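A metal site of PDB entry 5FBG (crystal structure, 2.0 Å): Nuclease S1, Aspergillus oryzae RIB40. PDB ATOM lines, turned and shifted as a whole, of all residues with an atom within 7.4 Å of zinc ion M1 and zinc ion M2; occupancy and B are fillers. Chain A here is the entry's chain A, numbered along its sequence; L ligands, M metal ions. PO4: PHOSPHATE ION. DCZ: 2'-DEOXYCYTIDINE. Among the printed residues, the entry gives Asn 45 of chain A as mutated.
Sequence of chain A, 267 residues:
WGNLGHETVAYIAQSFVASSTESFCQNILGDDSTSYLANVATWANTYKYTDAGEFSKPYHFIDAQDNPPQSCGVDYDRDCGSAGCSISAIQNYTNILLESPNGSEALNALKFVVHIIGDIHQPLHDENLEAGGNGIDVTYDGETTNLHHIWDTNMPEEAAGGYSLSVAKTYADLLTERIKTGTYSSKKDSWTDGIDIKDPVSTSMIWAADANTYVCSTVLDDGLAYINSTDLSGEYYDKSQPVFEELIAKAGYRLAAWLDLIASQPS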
ATOM      1  N   TRP A   1      17.394 -17.929   9.296  1.00  0.00           N
ATOM      2  CA  TRP A   1      16.541 -16.796   9.126  1.00  0.00           C
ATOM      3  C   TRP A   1      15.337 -16.918  10.053  1.00  0.00           C
ATOM      4  O   TRP A   1      14.938 -18.027  10.426  1.00  0.00           O
ATOM      5  CB  TRP A   1      16.047 -16.613   7.694  1.00  0.00           C
ATOM      6  CG  TRP A   1      17.149 -16.636   6.669  1.00  0.00           C
ATOM      7  CD1 TRP A   1      17.473 -17.659   5.876  1.00  0.00           C
ATOM      8  CD2 TRP A   1      18.072 -15.557   6.354  1.00  0.00           C
ATOM      9  NE1 TRP A   1      18.495 -17.285   5.022  1.00  0.00           N
ATOM     10  CE2 TRP A   1      18.872 -15.991   5.311  1.00  0.00           C
ATOM     11  CE3 TRP A   1      18.250 -14.257   6.855  1.00  0.00           C
ATOM     12  CZ2 TRP A   1      19.921 -15.197   4.776  1.00  0.00           C
ATOM     13  CZ3 TRP A   1      19.258 -13.458   6.309  1.00  0.00           C
ATOM     14  CH2 TRP A   1      20.089 -13.929   5.280  1.00  0.00           C
ATOM     15  N   GLY A   2      14.713 -15.765  10.290  1.00  0.00           N
ATOM     16  CA  GLY A   2      13.378 -15.715  10.866  1.00  0.00           C
ATOM     17  C   GLY A   2      12.331 -16.038   9.783  1.00  0.00           C
ATOM     18  O   GLY A   2      12.655 -16.432   8.654  1.00  0.00           O
ATOM     19  N   ASN A   3      11.074 -15.899  10.154  1.00  0.00           N
ATOM     20  CA  ASN A   3       9.958 -16.328   9.261  1.00  0.00           C
ATOM     21  C   ASN A   3       9.939 -15.584   7.951  1.00  0.00           C
ATOM     22  O   ASN A   3       9.792 -16.190   6.932  1.00  0.00           O
ATOM     23  CB  ASN A   3       8.628 -16.184   9.982  1.00  0.00           C
ATOM     24  CG  ASN A   3       8.485 -17.195  11.119  1.00  0.00           C
ATOM     25  OD1 ASN A   3       9.355 -18.075  11.343  1.00  0.00           O
ATOM     26  ND2 ASN A   3       7.416 -17.086  11.833  1.00  0.00           N
ATOM     27  N   GLY A   5      12.412 -14.181   6.281  1.00  0.00           N
ATOM     28  CA  GLY A   5      13.492 -14.684   5.408  1.00  0.00           C
ATOM     29  C   GLY A   5      13.169 -16.010   4.782  1.00  0.00           C
ATOM     30  O   GLY A   5      13.325 -16.188   3.589  1.00  0.00           O
ATOM     31  N   HIS A   6      12.717 -16.971   5.583  1.00  0.00           N
ATOM     32  CA  HIS A   6      12.369 -18.282   5.072  1.00  0.00           C
ATOM     33  C   HIS A   6      11.237 -18.238   4.041  1.00  0.00           C
ATOM     34  O   HIS A   6      11.294 -18.953   3.050  1.00  0.00           O
ATOM     35  CB  HIS A   6      12.014 -19.295   6.174  1.00  0.00           C
ATOM     36  CG  HIS A   6      13.212 -19.761   6.926  1.00  0.00           C
ATOM     37  ND1 HIS A   6      14.106 -20.636   6.396  1.00  0.00           N
ATOM     38  CD2 HIS A   6      13.704 -19.393   8.143  1.00  0.00           C
ATOM     39  CE1 HIS A   6      15.131 -20.783   7.224  1.00  0.00           C
ATOM     40  NE2 HIS A   6      14.916 -20.034   8.283  1.00  0.00           N
ATOM     41  N   ALA A  41       7.728 -23.221   5.102  1.00  0.00           N
ATOM     42  CA  ALA A  41       9.143 -22.812   5.131  1.00  0.00           C
ATOM     43  C   ALA A  41       9.710 -22.635   6.558  1.00  0.00           C
ATOM     44  O   ALA A  41      10.938 -22.568   6.720  1.00  0.00           O
ATOM     45  CB  ALA A  41       9.348 -21.520   4.339  1.00  0.00           C
ATOM     46  N   THR A  42       8.823 -22.498   7.547  1.00  0.00           N
ATOM     47  CA  THR A  42       9.248 -22.383   8.918  1.00  0.00           C
ATOM     48  C   THR A  42       9.044 -23.662   9.716  1.00  0.00           C
ATOM     49  O   THR A  42       9.452 -23.732  10.884  1.00  0.00           O
ATOM     50  CB  THR A  42       8.569 -21.221   9.666  1.00  0.00           C
ATOM     51  OG1 THR A  42       7.186 -21.530   9.918  1.00  0.00           O
ATOM     52  CG2 THR A  42       8.653 -19.953   8.856  1.00  0.00           C
ATOM     53  N   ALA A  44      10.430 -26.522  10.019  1.00  0.00           N
ATOM     54  CA  ALA A  44      11.548 -27.194  10.678  1.00  0.00           C
ATOM     55  C   ALA A  44      11.860 -26.542  12.019  1.00  0.00           C
ATOM     56  O   ALA A  44      12.252 -27.250  12.972  1.00  0.00           O
ATOM     57  CB  ALA A  44      12.748 -27.247   9.803  1.00  0.00           C
ATOM     58  N   ASN A  45      11.684 -25.209  12.073  1.00  0.00           N
ATOM     59  CA  ASN A  45      11.810 -24.518  13.318  1.00  0.00           C
ATOM     60  C   ASN A  45      10.757 -24.950  14.319  1.00  0.00           C
ATOM     61  O   ASN A  45      11.069 -25.280  15.450  1.00  0.00           O
ATOM     62  CB  ASN A  45      11.821 -22.994  13.164  1.00  0.00           C
ATOM     63  CG  ASN A  45      13.159 -22.467  12.688  1.00  0.00           C
ATOM     64  OD1 ASN A  45      14.134 -23.191  12.656  1.00  0.00           O
ATOM     65  ND2 ASN A  45      13.173 -21.237  12.279  1.00  0.00           N
ATOM     66  N   LYS A  48      11.567 -28.574  15.616  1.00  0.00           N
ATOM     67  CA  LYS A  48      12.745 -28.757  16.497  1.00  0.00           C
ATOM     68  C   LYS A  48      12.413 -28.493  18.009  1.00  0.00           C
ATOM     69  O   LYS A  48      13.147 -28.980  18.886  1.00  0.00           O
ATOM     70  CB  LYS A  48      13.938 -27.929  16.051  1.00  0.00           C
ATOM     71  CG  LYS A  48      13.845 -26.456  16.423  1.00  0.00           C
ATOM     72  CD  LYS A  48      14.934 -25.698  15.673  1.00  0.00           C
ATOM     73  CE  LYS A  48      15.067 -24.224  15.949  1.00  0.00           C
ATOM     74  NZ  LYS A  48      16.069 -23.568  15.018  1.00  0.00           N
ATOM     75  N   LYS A  57      17.409 -30.154  16.031  1.00  0.00           N
ATOM     76  CA  LYS A  57      17.963 -28.836  16.259  1.00  0.00           C
ATOM     77  C   LYS A  57      19.325 -28.538  15.576  1.00  0.00           C
ATOM     78  O   LYS A  57      19.519 -27.457  15.082  1.00  0.00           O
ATOM     79  CB  LYS A  57      18.110 -28.528  17.777  1.00  0.00           C
ATOM     80  CG  LYS A  57      16.802 -28.103  18.441  1.00  0.00           C
ATOM     81  CD  LYS A  57      16.953 -27.957  19.962  1.00  0.00           C
ATOM     82  CE  LYS A  57      15.591 -27.598  20.526  1.00  0.00           C
ATOM     83  NZ  LYS A  57      15.656 -27.338  21.991  1.00  0.00           N
ATOM     84  N   TYR A  59      20.488 -29.563  12.889  1.00  0.00           N
ATOM     85  CA  TYR A  59      20.368 -29.641  11.424  1.00  0.00           C
ATOM     86  C   TYR A  59      20.208 -28.279  10.780  1.00  0.00           C
ATOM     87  O   TYR A  59      20.188 -28.169   9.589  1.00  0.00           O
ATOM     88  CB  TYR A  59      19.206 -30.565  11.006  1.00  0.00           C
ATOM     89  CG  TYR A  59      19.228 -32.016  11.455  1.00  0.00           C
ATOM     90  CD1 TYR A  59      20.332 -32.593  12.084  1.00  0.00           C
ATOM     91  CD2 TYR A  59      18.141 -32.830  11.184  1.00  0.00           C
ATOM     92  CE1 TYR A  59      20.348 -33.944  12.435  1.00  0.00           C
ATOM     93  CE2 TYR A  59      18.134 -34.162  11.506  1.00  0.00           C
ATOM     94  CZ  TYR A  59      19.228 -34.730  12.132  1.00  0.00           C
ATOM     95  OH  TYR A  59      19.172 -36.067  12.447  1.00  0.00           O
ATOM     96  N   HIS A  60      20.105 -27.231  11.586  1.00  0.00           N
ATOM     97  CA  HIS A  60      19.892 -25.892  11.073  1.00  0.00           C
ATOM     98  C   HIS A  60      21.142 -25.098  10.769  1.00  0.00           C
ATOM     99  O   HIS A  60      21.060 -23.951  10.203  1.00  0.00           O
ATOM    100  CB  HIS A  60      19.013 -25.112  12.090  1.00  0.00           C
ATOM    101  CG  HIS A  60      17.638 -25.676  12.180  1.00  0.00           C
ATOM    102  ND1 HIS A  60      16.521 -24.977  11.760  1.00  0.00           N
ATOM    103  CD2 HIS A  60      17.218 -26.933  12.487  1.00  0.00           C
ATOM    104  CE1 HIS A  60      15.462 -25.752  11.885  1.00  0.00           C
ATOM    105  NE2 HIS A  60      15.857 -26.959  12.280  1.00  0.00           N
ATOM    106  N   PHE A  61      22.303 -25.658  11.128  1.00  0.00           N
ATOM    107  CA  PHE A  61      23.573 -24.916  11.009  1.00  0.00           C
ATOM    108  C   PHE A  61      24.738 -25.863  10.869  1.00  0.00           C
ATOM    109  O   PHE A  61      24.640 -27.096  11.000  1.00  0.00           O
ATOM    110  CB  PHE A  61      23.731 -23.930  12.202  1.00  0.00           C
ATOM    111  CG  PHE A  61      23.619 -24.607  13.532  1.00  0.00           C
ATOM    112  CD1 PHE A  61      24.722 -25.256  14.094  1.00  0.00           C
ATOM    113  CD2 PHE A  61      22.401 -24.602  14.220  1.00  0.00           C
ATOM    114  CE1 PHE A  61      24.614 -25.898  15.300  1.00  0.00           C
ATOM    115  CE2 PHE A  61      22.274 -25.237  15.446  1.00  0.00           C
ATOM    116  CZ  PHE A  61      23.365 -25.894  15.990  1.00  0.00           C
ATOM    117  N   HIS A 115      13.492 -25.402   4.275  1.00  0.00           N
ATOM    118  CA  HIS A 115      13.949 -24.575   5.372  1.00  0.00           C
ATOM    119  C   HIS A 115      15.501 -24.482   5.413  1.00  0.00           C
ATOM    120  O   HIS A 115      16.056 -23.410   5.550  1.00  0.00           O
ATOM    121  CB  HIS A 115      13.435 -25.121   6.717  1.00  0.00           C
ATOM    122  CG  HIS A 115      13.845 -24.286   7.888  1.00  0.00           C
ATOM    123  ND1 HIS A 115      13.131 -23.204   8.301  1.00  0.00           N
ATOM    124  CD2 HIS A 115      14.918 -24.365   8.718  1.00  0.00           C
ATOM    125  CE1 HIS A 115      13.721 -22.645   9.344  1.00  0.00           C
ATOM    126  NE2 HIS A 115      14.800 -23.341   9.622  1.00  0.00           N
ATOM    127  N   ILE A 116      16.150 -25.628   5.291  1.00  0.00           N
ATOM    128  CA  ILE A 116      17.578 -25.731   5.573  1.00  0.00           C
ATOM    129  C   ILE A 116      18.411 -25.093   4.438  1.00  0.00           C
ATOM    130  O   ILE A 116      19.361 -24.421   4.721  1.00  0.00           O
ATOM    131  CB  ILE A 116      17.994 -27.167   5.891  1.00  0.00           C
ATOM    132  CG1 ILE A 116      17.356 -27.601   7.202  1.00  0.00           C
ATOM    133  CG2 ILE A 116      19.503 -27.253   5.999  1.00  0.00           C
ATOM    134  CD1 ILE A 116      17.500 -29.096   7.458  1.00  0.00           C
ATOM    135  N   GLY A 118      17.465 -22.534   2.983  1.00  0.00           N
ATOM    136  CA  GLY A 118      17.387 -21.133   3.441  1.00  0.00           C
ATOM    137  C   GLY A 118      18.465 -20.862   4.502  1.00  0.00           C
ATOM    138  O   GLY A 118      19.240 -19.892   4.403  1.00  0.00           O
ATOM    139  N   ASP A 119      18.453 -21.663   5.555  1.00  0.00           N
ATOM    140  CA  ASP A 119      19.327 -21.422   6.745  1.00  0.00           C
ATOM    141  C   ASP A 119      20.832 -21.432   6.396  1.00  0.00           C
ATOM    142  O   ASP A 119      21.579 -20.592   6.887  1.00  0.00           O
ATOM    143  CB  ASP A 119      19.070 -22.466   7.814  1.00  0.00           C
ATOM    144  CG  ASP A 119      18.112 -22.049   8.882  1.00  0.00           C
ATOM    145  OD1 ASP A 119      17.658 -20.864   8.924  1.00  0.00           O
ATOM    146  OD2 ASP A 119      17.779 -22.971   9.661  1.00  0.00           O
ATOM    147  N   ILE A 120      21.227 -22.330   5.481  1.00  0.00           N
ATOM    148  CA  ILE A 120      22.606 -22.391   4.973  1.00  0.00           C
ATOM    149  C   ILE A 120      23.094 -21.045   4.484  1.00  0.00           C
ATOM    150  O   ILE A 120      24.295 -20.700   4.615  1.00  0.00           O
ATOM    151  CB  ILE A 120      22.778 -23.509   3.922  1.00  0.00           C
ATOM    152  CG1 ILE A 120      22.671 -24.883   4.615  1.00  0.00           C
ATOM    153  CG2 ILE A 120      24.120 -23.359   3.151  1.00  0.00           C
ATOM    154  CD1 ILE A 120      22.487 -26.025   3.643  1.00  0.00           C
ATOM    155  N   GLN A 122      22.281 -18.039   5.534  1.00  0.00           N
ATOM    156  CA  GLN A 122      22.410 -17.045   6.572  1.00  0.00           C
ATOM    157  C   GLN A 122      23.834 -17.254   7.139  1.00  0.00           C
ATOM    158  O   GLN A 122      24.085 -18.305   7.711  1.00  0.00           O
ATOM    159  CB  GLN A 122      21.346 -17.254   7.662  1.00  0.00           C
ATOM    160  CG  GLN A 122      20.968 -16.017   8.452  1.00  0.00           C
ATOM    161  CD  GLN A 122      22.032 -15.590   9.523  1.00  0.00           C
ATOM    162  OE1 GLN A 122      23.169 -15.253   9.158  1.00  0.00           O
ATOM    163  NE2 GLN A 122      21.652 -15.586  10.767  1.00  0.00           N
ATOM    164  N   HIS A 125      24.719 -19.028  10.360  1.00  0.00           N
ATOM    165  CA  HIS A 125      24.431 -20.495  10.393  1.00  0.00           C
ATOM    166  C   HIS A 125      25.565 -21.326   9.866  1.00  0.00           C
ATOM    167  O   HIS A 125      25.445 -22.545   9.752  1.00  0.00           O
ATOM    168  CB  HIS A 125      23.164 -20.750   9.539  1.00  0.00           C
ATOM    169  CG  HIS A 125      21.891 -20.436  10.271  1.00  0.00           C
ATOM    170  ND1 HIS A 125      21.030 -21.430  10.678  1.00  0.00           N
ATOM    171  CD2 HIS A 125      21.377 -19.279  10.710  1.00  0.00           C
ATOM    172  CE1 HIS A 125      20.040 -20.887  11.356  1.00  0.00           C
ATOM    173  NE2 HIS A 125      20.214 -19.590  11.368  1.00  0.00           N
ATOM    174  N   HIS A 148      23.122 -12.826  16.025  1.00  0.00           N
ATOM    175  CA  HIS A 148      22.473 -13.830  15.218  1.00  0.00           C
ATOM    176  C   HIS A 148      21.034 -13.352  14.874  1.00  0.00           C
ATOM    177  O   HIS A 148      20.588 -13.412  13.709  1.00  0.00           O
ATOM    178  CB  HIS A 148      22.385 -15.147  15.940  1.00  0.00           C
ATOM    179  CG  HIS A 148      21.837 -16.249  15.096  1.00  0.00           C
ATOM    180  ND1 HIS A 148      22.649 -17.199  14.503  1.00  0.00           N
ATOM    181  CD2 HIS A 148      20.571 -16.531  14.690  1.00  0.00           C
ATOM    182  CE1 HIS A 148      21.890 -18.030  13.779  1.00  0.00           C
ATOM    183  NE2 HIS A 148      20.638 -17.663  13.921  1.00  0.00           N
ATOM    184  N   ASP A 152      19.007 -12.816  11.315  1.00  0.00           N
ATOM    185  CA  ASP A 152      17.859 -13.672  11.031  1.00  0.00           C
ATOM    186  C   ASP A 152      16.595 -12.821  10.726  1.00  0.00           C
ATOM    187  O   ASP A 152      15.855 -13.120   9.795  1.00  0.00           O
ATOM    188  CB  ASP A 152      17.536 -14.594  12.213  1.00  0.00           C
ATOM    189  CG  ASP A 152      18.121 -15.998  12.107  1.00  0.00           C
ATOM    190  OD1 ASP A 152      18.907 -16.343  11.223  1.00  0.00           O
ATOM    191  OD2 ASP A 152      17.822 -16.779  13.032  1.00  0.00           O
HETATM  192  P   PO4 L   1      16.605 -20.661  12.679  1.00  0.00           P
HETATM  193  O1  PO4 L   1      15.926 -20.522  11.340  1.00  0.00           O
HETATM  194  O2  PO4 L   1      17.161 -22.086  12.780  1.00  0.00           O
HETATM  195  O3  PO4 L   1      17.675 -19.641  12.896  1.00  0.00           O
HETATM  196  O4  PO4 L   1      15.741 -20.538  13.914  1.00  0.00           O
HETATM  197  N1  DCZ L   2      21.856 -21.333  15.756  1.00  0.00           N
HETATM  198  C2  DCZ L   2      22.934 -21.355  14.862  1.00  0.00           C
HETATM  199  N3  DCZ L   2      24.147 -21.838  15.294  1.00  0.00           N
HETATM  200  C4  DCZ L   2      24.278 -22.325  16.533  1.00  0.00           C
HETATM  201  C5  DCZ L   2      23.182 -22.306  17.472  1.00  0.00           C
HETATM  202  C6  DCZ L   2      22.009 -21.792  17.058  1.00  0.00           C
HETATM  203  O2  DCZ L   2      22.740 -21.012  13.699  1.00  0.00           O
HETATM  204  N4  DCZ L   2      25.437 -22.844  16.885  1.00  0.00           N
HETATM  205  C1' DCZ L   2      20.531 -20.903  15.264  1.00  0.00           C
HETATM  206  C2' DCZ L   2      19.419 -21.945  15.429  1.00  0.00           C
HETATM  207  C3' DCZ L   2      18.617 -21.445  16.651  1.00  0.00           C
HETATM  208  C4' DCZ L   2      18.821 -19.943  16.553  1.00  0.00           C
HETATM  209  O4' DCZ L   2      20.153 -19.771  16.012  1.00  0.00           O
HETATM  210  O3' DCZ L   2      17.199 -21.640  16.639  1.00  0.00           O
HETATM  211  C5' DCZ L   2      18.688 -19.162  17.856  1.00  0.00           C
HETATM  212  O5' DCZ L   2      18.581 -17.772  17.503  1.00  0.00           O
HETATM  213 ZN    ZN M   1      16.212 -19.659   9.770  1.00  0.00          ZN
HETATM  214 ZN    ZN M   2      16.240 -23.028  11.152  1.00  0.00          ZN
HETATM  215 ZN    ZN M   3      19.063 -18.396  12.720  1.00  0.00          ZN
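Lys 48 touches zinc ion M2. Of the 23 residues printed, 5 come within 4 Å of zinc ion M2. The nearest printed residue that does not touch zinc ion M2 is His 6 (4.4 Å).
The side-chain amino group (NZ) of Lys 48 is in hydrogen-bond range of an oxygen (O3') of DCZ L2 (2.8 Å). An oxygen (O2) of DCZ L2 lies within hydrogen-bond range of a ring nitrogen (ND1) of His 125, 3.5 Å away. O4' of DCZ L2 lies close to NE2 of His 148 (3.0 Å).
ND1 of His 6 lies close to ND1 of His 115, at 3.3 Å. The backbone carbonyl oxygen of His 60 is in hydrogen-bond range of a ring nitrogen (ND1) of His 125 (2.6 Å). A ring nitrogen (ND1) of His 115 sits at hydrogen-bond distance from the backbone carbonyl oxygen of Ala 41, 2.8 Å away. NE1 of Trp 1 is in hydrogen-bond range of O of Gly 118 (2.8 Å). The side-chain amino group of Lys 48 sits close to the side-chain amide oxygen of Asn 45 (3.1 Å).
Within 4 Å of zinc ion M1: Trp 1, His 6, His 115 and Asp 119. Along chain A the residues within 4 Å of zinc ion M1 span positions 1 to 119.
Zinc ion M1 is bound by O1 of PO4 L1, NE2 of His 6, OD1 of Asp 119, N of Trp 1 and O of Trp 1.
ND1 of His 60 binds zinc ion M2, 2.1 Å away. Zinc ion M2 is bound by O2 of PO4 L1 (2.1 Å). Zinc ion M2 is bound by NE2 of His 115 (2.1 Å). Zinc ion M2 is bound by OD2 of Asp 119 (2.1 Å). An oxygen (O1) of PO4 L1 binds zinc ion M2 (2.5 Å). OD1 of Asn 45 binds zinc ion M2, at 2.6 Å. Zinc ion M2 has six donor atoms within binding distance.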
